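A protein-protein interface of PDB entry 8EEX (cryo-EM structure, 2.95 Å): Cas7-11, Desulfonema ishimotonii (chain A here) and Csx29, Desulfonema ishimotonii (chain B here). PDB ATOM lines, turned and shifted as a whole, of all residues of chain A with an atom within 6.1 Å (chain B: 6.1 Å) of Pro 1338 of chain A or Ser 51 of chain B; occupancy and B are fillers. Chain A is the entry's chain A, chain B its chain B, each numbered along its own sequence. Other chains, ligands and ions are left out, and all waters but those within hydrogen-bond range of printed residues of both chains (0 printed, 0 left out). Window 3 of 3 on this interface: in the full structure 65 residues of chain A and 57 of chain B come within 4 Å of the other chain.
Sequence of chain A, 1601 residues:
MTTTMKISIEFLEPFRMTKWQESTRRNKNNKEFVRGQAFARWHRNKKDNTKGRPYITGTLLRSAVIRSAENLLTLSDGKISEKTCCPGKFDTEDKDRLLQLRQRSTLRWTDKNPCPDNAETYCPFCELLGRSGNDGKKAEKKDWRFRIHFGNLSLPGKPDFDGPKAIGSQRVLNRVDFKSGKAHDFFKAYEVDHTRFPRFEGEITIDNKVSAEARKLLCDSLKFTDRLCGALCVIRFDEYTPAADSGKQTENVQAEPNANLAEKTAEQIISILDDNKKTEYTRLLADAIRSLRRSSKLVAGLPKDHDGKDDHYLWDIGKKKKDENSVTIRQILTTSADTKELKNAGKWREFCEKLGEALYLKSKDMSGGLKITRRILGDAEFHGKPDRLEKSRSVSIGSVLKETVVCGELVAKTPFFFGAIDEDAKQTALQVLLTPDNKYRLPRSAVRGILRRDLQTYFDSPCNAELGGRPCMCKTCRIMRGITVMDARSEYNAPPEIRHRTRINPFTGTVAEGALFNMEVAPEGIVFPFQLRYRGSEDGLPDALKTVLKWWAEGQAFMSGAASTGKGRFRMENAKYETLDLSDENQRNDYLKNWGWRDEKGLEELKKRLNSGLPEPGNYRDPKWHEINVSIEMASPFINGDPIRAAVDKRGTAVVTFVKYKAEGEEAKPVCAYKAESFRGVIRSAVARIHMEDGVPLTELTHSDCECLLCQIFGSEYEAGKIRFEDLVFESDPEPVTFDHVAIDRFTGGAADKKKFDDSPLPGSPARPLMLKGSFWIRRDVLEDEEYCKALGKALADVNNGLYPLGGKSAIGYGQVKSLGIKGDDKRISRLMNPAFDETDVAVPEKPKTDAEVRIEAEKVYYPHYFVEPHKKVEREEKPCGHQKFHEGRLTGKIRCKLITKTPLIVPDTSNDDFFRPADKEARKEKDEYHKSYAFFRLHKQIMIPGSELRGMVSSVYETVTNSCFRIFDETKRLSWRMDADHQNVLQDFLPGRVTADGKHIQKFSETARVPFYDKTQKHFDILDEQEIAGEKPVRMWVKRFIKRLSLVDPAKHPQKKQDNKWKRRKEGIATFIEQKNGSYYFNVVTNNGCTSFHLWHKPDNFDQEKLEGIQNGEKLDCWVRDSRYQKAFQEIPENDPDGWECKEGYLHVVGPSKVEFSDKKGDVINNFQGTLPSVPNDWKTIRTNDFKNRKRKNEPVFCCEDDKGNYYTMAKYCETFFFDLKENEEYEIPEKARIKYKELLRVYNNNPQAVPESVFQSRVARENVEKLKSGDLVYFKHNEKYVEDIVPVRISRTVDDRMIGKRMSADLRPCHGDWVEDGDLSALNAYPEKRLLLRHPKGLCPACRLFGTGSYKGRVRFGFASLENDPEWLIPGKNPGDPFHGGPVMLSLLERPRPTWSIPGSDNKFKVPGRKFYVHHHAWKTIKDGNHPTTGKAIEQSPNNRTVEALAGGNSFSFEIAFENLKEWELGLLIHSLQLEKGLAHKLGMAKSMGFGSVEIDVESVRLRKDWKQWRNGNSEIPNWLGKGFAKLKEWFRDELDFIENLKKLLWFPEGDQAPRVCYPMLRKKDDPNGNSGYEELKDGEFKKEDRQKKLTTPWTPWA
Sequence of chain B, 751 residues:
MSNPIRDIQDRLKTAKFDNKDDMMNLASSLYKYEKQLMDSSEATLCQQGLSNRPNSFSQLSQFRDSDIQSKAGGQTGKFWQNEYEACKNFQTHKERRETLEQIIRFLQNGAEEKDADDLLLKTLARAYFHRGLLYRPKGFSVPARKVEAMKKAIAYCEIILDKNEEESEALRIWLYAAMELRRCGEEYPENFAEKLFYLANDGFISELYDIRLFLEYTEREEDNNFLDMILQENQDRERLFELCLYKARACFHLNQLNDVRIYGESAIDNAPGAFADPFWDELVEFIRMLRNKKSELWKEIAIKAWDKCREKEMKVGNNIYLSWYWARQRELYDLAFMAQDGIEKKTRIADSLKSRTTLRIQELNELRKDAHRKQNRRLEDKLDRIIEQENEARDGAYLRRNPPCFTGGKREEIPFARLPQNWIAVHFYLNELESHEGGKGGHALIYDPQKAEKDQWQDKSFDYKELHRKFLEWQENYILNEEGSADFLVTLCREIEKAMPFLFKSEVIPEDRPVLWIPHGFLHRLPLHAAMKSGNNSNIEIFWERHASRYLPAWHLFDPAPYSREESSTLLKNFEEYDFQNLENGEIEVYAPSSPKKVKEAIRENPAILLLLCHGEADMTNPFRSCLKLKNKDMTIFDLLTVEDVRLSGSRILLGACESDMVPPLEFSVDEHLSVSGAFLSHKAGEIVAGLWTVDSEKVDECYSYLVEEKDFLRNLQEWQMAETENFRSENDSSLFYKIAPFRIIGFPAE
The backbone NH of Leu 50 of chain B lies within hydrogen-bond range of the backbone carbonyl oxygen of Leu 1333 of chain A (3.0 Å).
O of His 1337 of chain A sits at hydrogen-bond distance from N of Gly 49 of chain B (2.9 Å).
O of Gly 1340 of chain A is in hydrogen-bond range of NH1 of Arg 876 of chain A, 3.1 Å away.
The backbone NH (N) of Lys 1339 of chain A lies close to a ring nitrogen (ND1) of His 1337 of chain A (3.1 Å).
The side-chain hydroxyl (OG) of Ser 56 of chain B lies within hydrogen-bond range of the backbone carbonyl oxygen (O) of Ser 51 of chain B, 2.9 Å away.
The side-chain amide oxygen (OE1) of Gln 9 of chain B sits at hydrogen-bond distance from the backbone NH (N) of Ser 51 of chain B (2.7 Å).
CD2 of Leu 1333 of chain A touches O of Gln 48 of chain B (3.8 Å).
Arg 1336 of chain A touches Gln 48 of chain B.
Arg 1336 of chain A touches Gly 49 of chain B.
Arg 1336 of chain A touches Arg 53 of chain B.
CA of Gln 48 of chain B touches O of His 1337 of chain A, 3.4 Å away.
Arg 53 of chain B touches His 1337 of chain A (NH2 to CA, 3.8 Å).
CB of Gln 48 of chain B touches O of Pro 1338 of chain A, 3.4 Å away.
Pro 1338 of chain A touches Gly 49 of chain B (CA to O, 3.7 Å).
Leu 50 of chain B touches Pro 1338 of chain A (O to CG, 3.8 Å).
Gly 1340 of chain A touches Gln 48 of chain B.
Pro 1338 of chain A touches four residues of chain B.
Printed residues of chain B within 4 Å of Gly 1340 of chain A: Gln 48.
Printed residues of chain A within 4 Å of Gly 49 of chain B: Leu 1333 (3.3 Å), Arg 1336 (3.4 Å), His 1337 (2.9 Å) and Pro 1338 (3.7 Å).
Asn 52 of chain B touches none of the printed residues of chain A.
The nearest residue of chain B that does not touch Pro 1338 of chain A is Arg 53 of chain B (4.7 Å).
The nearest printed residue of chain A that does not touch Ser 51 of chain B is Leu 1333 of chain A (6.1 Å).
The nearest printed residue of chain A that does not touch Leu 50 of chain B is Arg 1336 of chain A (4.04 Å).
Hydrophobic or aromatic side chains of chain A that line the printed part of chain B: Leu 1333 and Pro 1338.
Of the 9 printed residues of chain B, 5 touch a printed residue of chain A.
Hydrophobic or aromatic side chains of chain B that line the printed part of chain A: Leu 50.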
ATOM      1  N   ARG A 876      -5.103  20.731   8.386  1.00  0.00           N
ATOM      2  CA  ARG A 876      -4.200  20.808   9.523  1.00  0.00           C
ATOM      3  C   ARG A 876      -2.748  20.842   9.062  1.00  0.00           C
ATOM      4  O   ARG A 876      -2.401  20.303   8.008  1.00  0.00           O
ATOM      5  CB  ARG A 876      -4.427  19.616  10.451  1.00  0.00           C
ATOM      6  CG  ARG A 876      -5.749  19.678  11.175  1.00  0.00           C
ATOM      7  CD  ARG A 876      -6.224  18.306  11.586  1.00  0.00           C
ATOM      8  NE  ARG A 876      -7.495  18.364  12.300  1.00  0.00           N
ATOM      9  CZ  ARG A 876      -7.623  18.522  13.611  1.00  0.00           C
ATOM     10  NH1 ARG A 876      -6.571  18.569  14.412  1.00  0.00           N
ATOM     11  NH2 ARG A 876      -8.841  18.620  14.135  1.00  0.00           N
ATOM     12  N   GLU A 878       1.348  20.367  10.675  1.00  0.00           N
ATOM     13  CA  GLU A 878       2.068  19.771  11.795  1.00  0.00           C
ATOM     14  C   GLU A 878       2.977  20.764  12.509  1.00  0.00           C
ATOM     15  O   GLU A 878       3.143  20.665  13.729  1.00  0.00           O
ATOM     16  CB  GLU A 878       2.881  18.575  11.299  1.00  0.00           C
ATOM     17  CG  GLU A 878       2.024  17.421  10.810  1.00  0.00           C
ATOM     18  CD  GLU A 878       2.833  16.306  10.188  1.00  0.00           C
ATOM     19  OE1 GLU A 878       4.033  16.521   9.913  1.00  0.00           O
ATOM     20  OE2 GLU A 878       2.270  15.211   9.973  1.00  0.00           O
ATOM     21  N   LEU A1333       1.408  13.554  23.864  1.00  0.00           N
ATOM     22  CA  LEU A1333       1.168  13.139  22.488  1.00  0.00           C
ATOM     23  C   LEU A1333      -0.118  12.342  22.314  1.00  0.00           C
ATOM     24  O   LEU A1333      -0.641  12.284  21.197  1.00  0.00           O
ATOM     25  CB  LEU A1333       2.350  12.318  21.970  1.00  0.00           C
ATOM     26  CG  LEU A1333       3.732  12.968  22.061  1.00  0.00           C
ATOM     27  CD1 LEU A1333       4.793  12.019  21.544  1.00  0.00           C
ATOM     28  CD2 LEU A1333       3.764  14.274  21.281  1.00  0.00           C
ATOM     29  N   ARG A1336      -2.977  15.055  21.464  1.00  0.00           N
ATOM     30  CA  ARG A1336      -2.825  15.919  20.301  1.00  0.00           C
ATOM     31  C   ARG A1336      -3.168  15.160  19.029  1.00  0.00           C
ATOM     32  O   ARG A1336      -2.920  13.955  18.927  1.00  0.00           O
ATOM     33  CB  ARG A1336      -1.402  16.470  20.228  1.00  0.00           C
ATOM     34  CG  ARG A1336      -1.049  17.340  21.412  1.00  0.00           C
ATOM     35  CD  ARG A1336       0.382  17.806  21.376  1.00  0.00           C
ATOM     36  NE  ARG A1336       0.719  18.564  22.574  1.00  0.00           N
ATOM     37  CZ  ARG A1336       1.823  19.281  22.725  1.00  0.00           C
ATOM     38  NH1 ARG A1336       2.739  19.352  21.776  1.00  0.00           N
ATOM     39  NH2 ARG A1336       2.011  19.948  23.859  1.00  0.00           N
ATOM     40  N   HIS A1337      -3.741  15.869  18.065  1.00  0.00           N
ATOM     41  CA  HIS A1337      -4.235  15.217  16.864  1.00  0.00           C
ATOM     42  C   HIS A1337      -3.048  14.780  16.001  1.00  0.00           C
ATOM     43  O   HIS A1337      -2.018  15.458  15.984  1.00  0.00           O
ATOM     44  CB  HIS A1337      -5.155  16.170  16.098  1.00  0.00           C
ATOM     45  CG  HIS A1337      -5.835  15.549  14.917  1.00  0.00           C
ATOM     46  ND1 HIS A1337      -5.228  15.400  13.691  1.00  0.00           N
ATOM     47  CD2 HIS A1337      -7.080  15.034  14.782  1.00  0.00           C
ATOM     48  CE1 HIS A1337      -6.066  14.822  12.851  1.00  0.00           C
ATOM     49  NE2 HIS A1337      -7.198  14.589  13.488  1.00  0.00           N
ATOM     50  N   PRO A1338      -3.145  13.639  15.278  1.00  0.00           N
ATOM     51  CA  PRO A1338      -1.977  13.144  14.534  1.00  0.00           C
ATOM     52  C   PRO A1338      -1.426  14.090  13.472  1.00  0.00           C
ATOM     53  O   PRO A1338      -0.277  13.941  13.048  1.00  0.00           O
ATOM     54  CB  PRO A1338      -2.508  11.862  13.881  1.00  0.00           C
ATOM     55  CG  PRO A1338      -3.539  11.391  14.801  1.00  0.00           C
ATOM     56  CD  PRO A1338      -4.222  12.633  15.279  1.00  0.00           C
ATOM     57  N   LYS A1339      -2.229  15.059  13.035  1.00  0.00           N
ATOM     58  CA  LYS A1339      -1.941  15.866  11.858  1.00  0.00           C
ATOM     59  C   LYS A1339      -1.716  17.340  12.167  1.00  0.00           C
ATOM     60  O   LYS A1339      -1.488  18.120  11.236  1.00  0.00           O
ATOM     61  CB  LYS A1339      -3.082  15.720  10.843  1.00  0.00           C
ATOM     62  CG  LYS A1339      -3.115  14.358  10.158  1.00  0.00           C
ATOM     63  CD  LYS A1339      -4.081  14.269   8.976  1.00  0.00           C
ATOM     64  CE  LYS A1339      -3.616  15.006   7.727  1.00  0.00           C
ATOM     65  NZ  LYS A1339      -4.007  16.439   7.676  1.00  0.00           N
ATOM     66  N   GLY A1340      -1.781  17.748  13.434  1.00  0.00           N
ATOM     67  CA  GLY A1340      -1.438  19.103  13.824  1.00  0.00           C
ATOM     68  C   GLY A1340      -2.606  20.038  14.075  1.00  0.00           C
ATOM     69  O   GLY A1340      -3.660  19.613  14.552  1.00  0.00           O
ATOM     70  N   GLN B   9       6.057   6.711  16.679  1.00  0.00           N
ATOM     71  CA  GLN B   9       4.927   6.031  16.052  1.00  0.00           C
ATOM     72  C   GLN B   9       5.374   4.748  15.368  1.00  0.00           C
ATOM     73  O   GLN B   9       4.694   3.718  15.449  1.00  0.00           O
ATOM     74  CB  GLN B   9       4.249   6.974  15.053  1.00  0.00           C
ATOM     75  CG  GLN B   9       2.925   6.474  14.495  1.00  0.00           C
ATOM     76  CD  GLN B   9       1.778   6.688  15.455  1.00  0.00           C
ATOM     77  OE1 GLN B   9       1.477   7.817  15.835  1.00  0.00           O
ATOM     78  NE2 GLN B   9       1.138   5.601  15.863  1.00  0.00           N
ATOM     79  N   LEU B  12       5.979   1.850  17.694  1.00  0.00           N
ATOM     80  CA  LEU B  12       4.760   1.243  18.212  1.00  0.00           C
ATOM     81  C   LEU B  12       4.025   0.413  17.172  1.00  0.00           C
ATOM     82  O   LEU B  12       3.351  -0.555  17.536  1.00  0.00           O
ATOM     83  CB  LEU B  12       3.818   2.325  18.752  1.00  0.00           C
ATOM     84  CG  LEU B  12       4.365   3.222  19.868  1.00  0.00           C
ATOM     85  CD1 LEU B  12       3.339   4.276  20.234  1.00  0.00           C
ATOM     86  CD2 LEU B  12       4.768   2.422  21.100  1.00  0.00           C
ATOM     87  N   GLN B  48       1.956  17.979  16.534  1.00  0.00           N
ATOM     88  CA  GLN B  48       1.061  16.845  16.346  1.00  0.00           C
ATOM     89  C   GLN B  48       1.247  15.799  17.446  1.00  0.00           C
ATOM     90  O   GLN B  48       2.120  15.909  18.308  1.00  0.00           O
ATOM     91  CB  GLN B  48       1.275  16.250  14.948  1.00  0.00           C
ATOM     92  CG  GLN B  48       2.483  15.326  14.752  1.00  0.00           C
ATOM     93  CD  GLN B  48       3.768  16.100  14.555  1.00  0.00           C
ATOM     94  OE1 GLN B  48       3.845  17.281  14.877  1.00  0.00           O
ATOM     95  NE2 GLN B  48       4.786  15.434  14.028  1.00  0.00           N
ATOM     96  N   GLY B  49       0.393  14.774  17.405  1.00  0.00           N
ATOM     97  CA  GLY B  49       0.411  13.697  18.377  1.00  0.00           C
ATOM     98  C   GLY B  49       0.490  12.322  17.747  1.00  0.00           C
ATOM     99  O   GLY B  49       0.921  12.189  16.598  1.00  0.00           O
ATOM    100  N   LEU B  50       0.080  11.291  18.485  1.00  0.00           N
ATOM    101  CA  LEU B  50       0.198   9.905  18.049  1.00  0.00           C
ATOM    102  C   LEU B  50      -1.112   9.387  17.474  1.00  0.00           C
ATOM    103  O   LEU B  50      -2.194   9.701  17.978  1.00  0.00           O
ATOM    104  CB  LEU B  50       0.630   9.003  19.208  1.00  0.00           C
ATOM    105  CG  LEU B  50       2.048   9.182  19.745  1.00  0.00           C
ATOM    106  CD1 LEU B  50       2.187   8.472  21.073  1.00  0.00           C
ATOM    107  CD2 LEU B  50       3.057   8.649  18.743  1.00  0.00           C
ATOM    108  N   SER B  51      -1.002   8.595  16.412  1.00  0.00           N
ATOM    109  CA  SER B  51      -2.154   7.912  15.847  1.00  0.00           C
ATOM    110  C   SER B  51      -2.463   6.642  16.635  1.00  0.00           C
ATOM    111  O   SER B  51      -1.645   6.144  17.413  1.00  0.00           O
ATOM    112  CB  SER B  51      -1.902   7.566  14.383  1.00  0.00           C
ATOM    113  OG  SER B  51      -3.100   7.174  13.743  1.00  0.00           O
ATOM    114  N   ASN B  52      -3.665   6.112  16.415  1.00  0.00           N
ATOM    115  CA  ASN B  52      -4.144   4.918  17.114  1.00  0.00           C
ATOM    116  C   ASN B  52      -4.040   5.098  18.626  1.00  0.00           C
ATOM    117  O   ASN B  52      -3.301   4.394  19.317  1.00  0.00           O
ATOM    118  CB  ASN B  52      -3.386   3.671  16.659  1.00  0.00           C
ATOM    119  CG  ASN B  52      -3.436   3.473  15.157  1.00  0.00           C
ATOM    120  OD1 ASN B  52      -4.487   3.626  14.536  1.00  0.00           O
ATOM    121  ND2 ASN B  52      -2.303   3.115  14.567  1.00  0.00           N
ATOM    122  N   ARG B  53      -4.788   6.076  19.137  1.00  0.00           N
ATOM    123  CA  ARG B  53      -4.734   6.447  20.553  1.00  0.00           C
ATOM    124  C   ARG B  53      -4.913   5.286  21.525  1.00  0.00           C
ATOM    125  O   ARG B  53      -4.053   5.119  22.400  1.00  0.00           O
ATOM    126  CB  ARG B  53      -5.802   7.518  20.808  1.00  0.00           C
ATOM    127  CG  ARG B  53      -5.393   8.912  20.389  1.00  0.00           C
ATOM    128  CD  ARG B  53      -6.474   9.901  20.755  1.00  0.00           C
ATOM    129  NE  ARG B  53      -6.123  11.286  20.452  1.00  0.00           N
ATOM    130  CZ  ARG B  53      -6.621  12.014  19.459  1.00  0.00           C
ATOM    131  NH1 ARG B  53      -7.389  11.485  18.519  1.00  0.00           N
ATOM    132  NH2 ARG B  53      -6.329  13.309  19.400  1.00  0.00           N
ATOM    133  N   SER B  56      -1.869   2.942  21.274  1.00  0.00           N
ATOM    134  CA  SER B  56      -0.649   3.599  21.733  1.00  0.00           C
ATOM    135  C   SER B  56      -0.631   3.720  23.251  1.00  0.00           C
ATOM    136  O   SER B  56       0.414   3.538  23.883  1.00  0.00           O
ATOM    137  CB  SER B  56      -0.520   4.977  21.087  1.00  0.00           C
ATOM    138  OG  SER B  56      -0.358   4.869  19.684  1.00  0.00           O
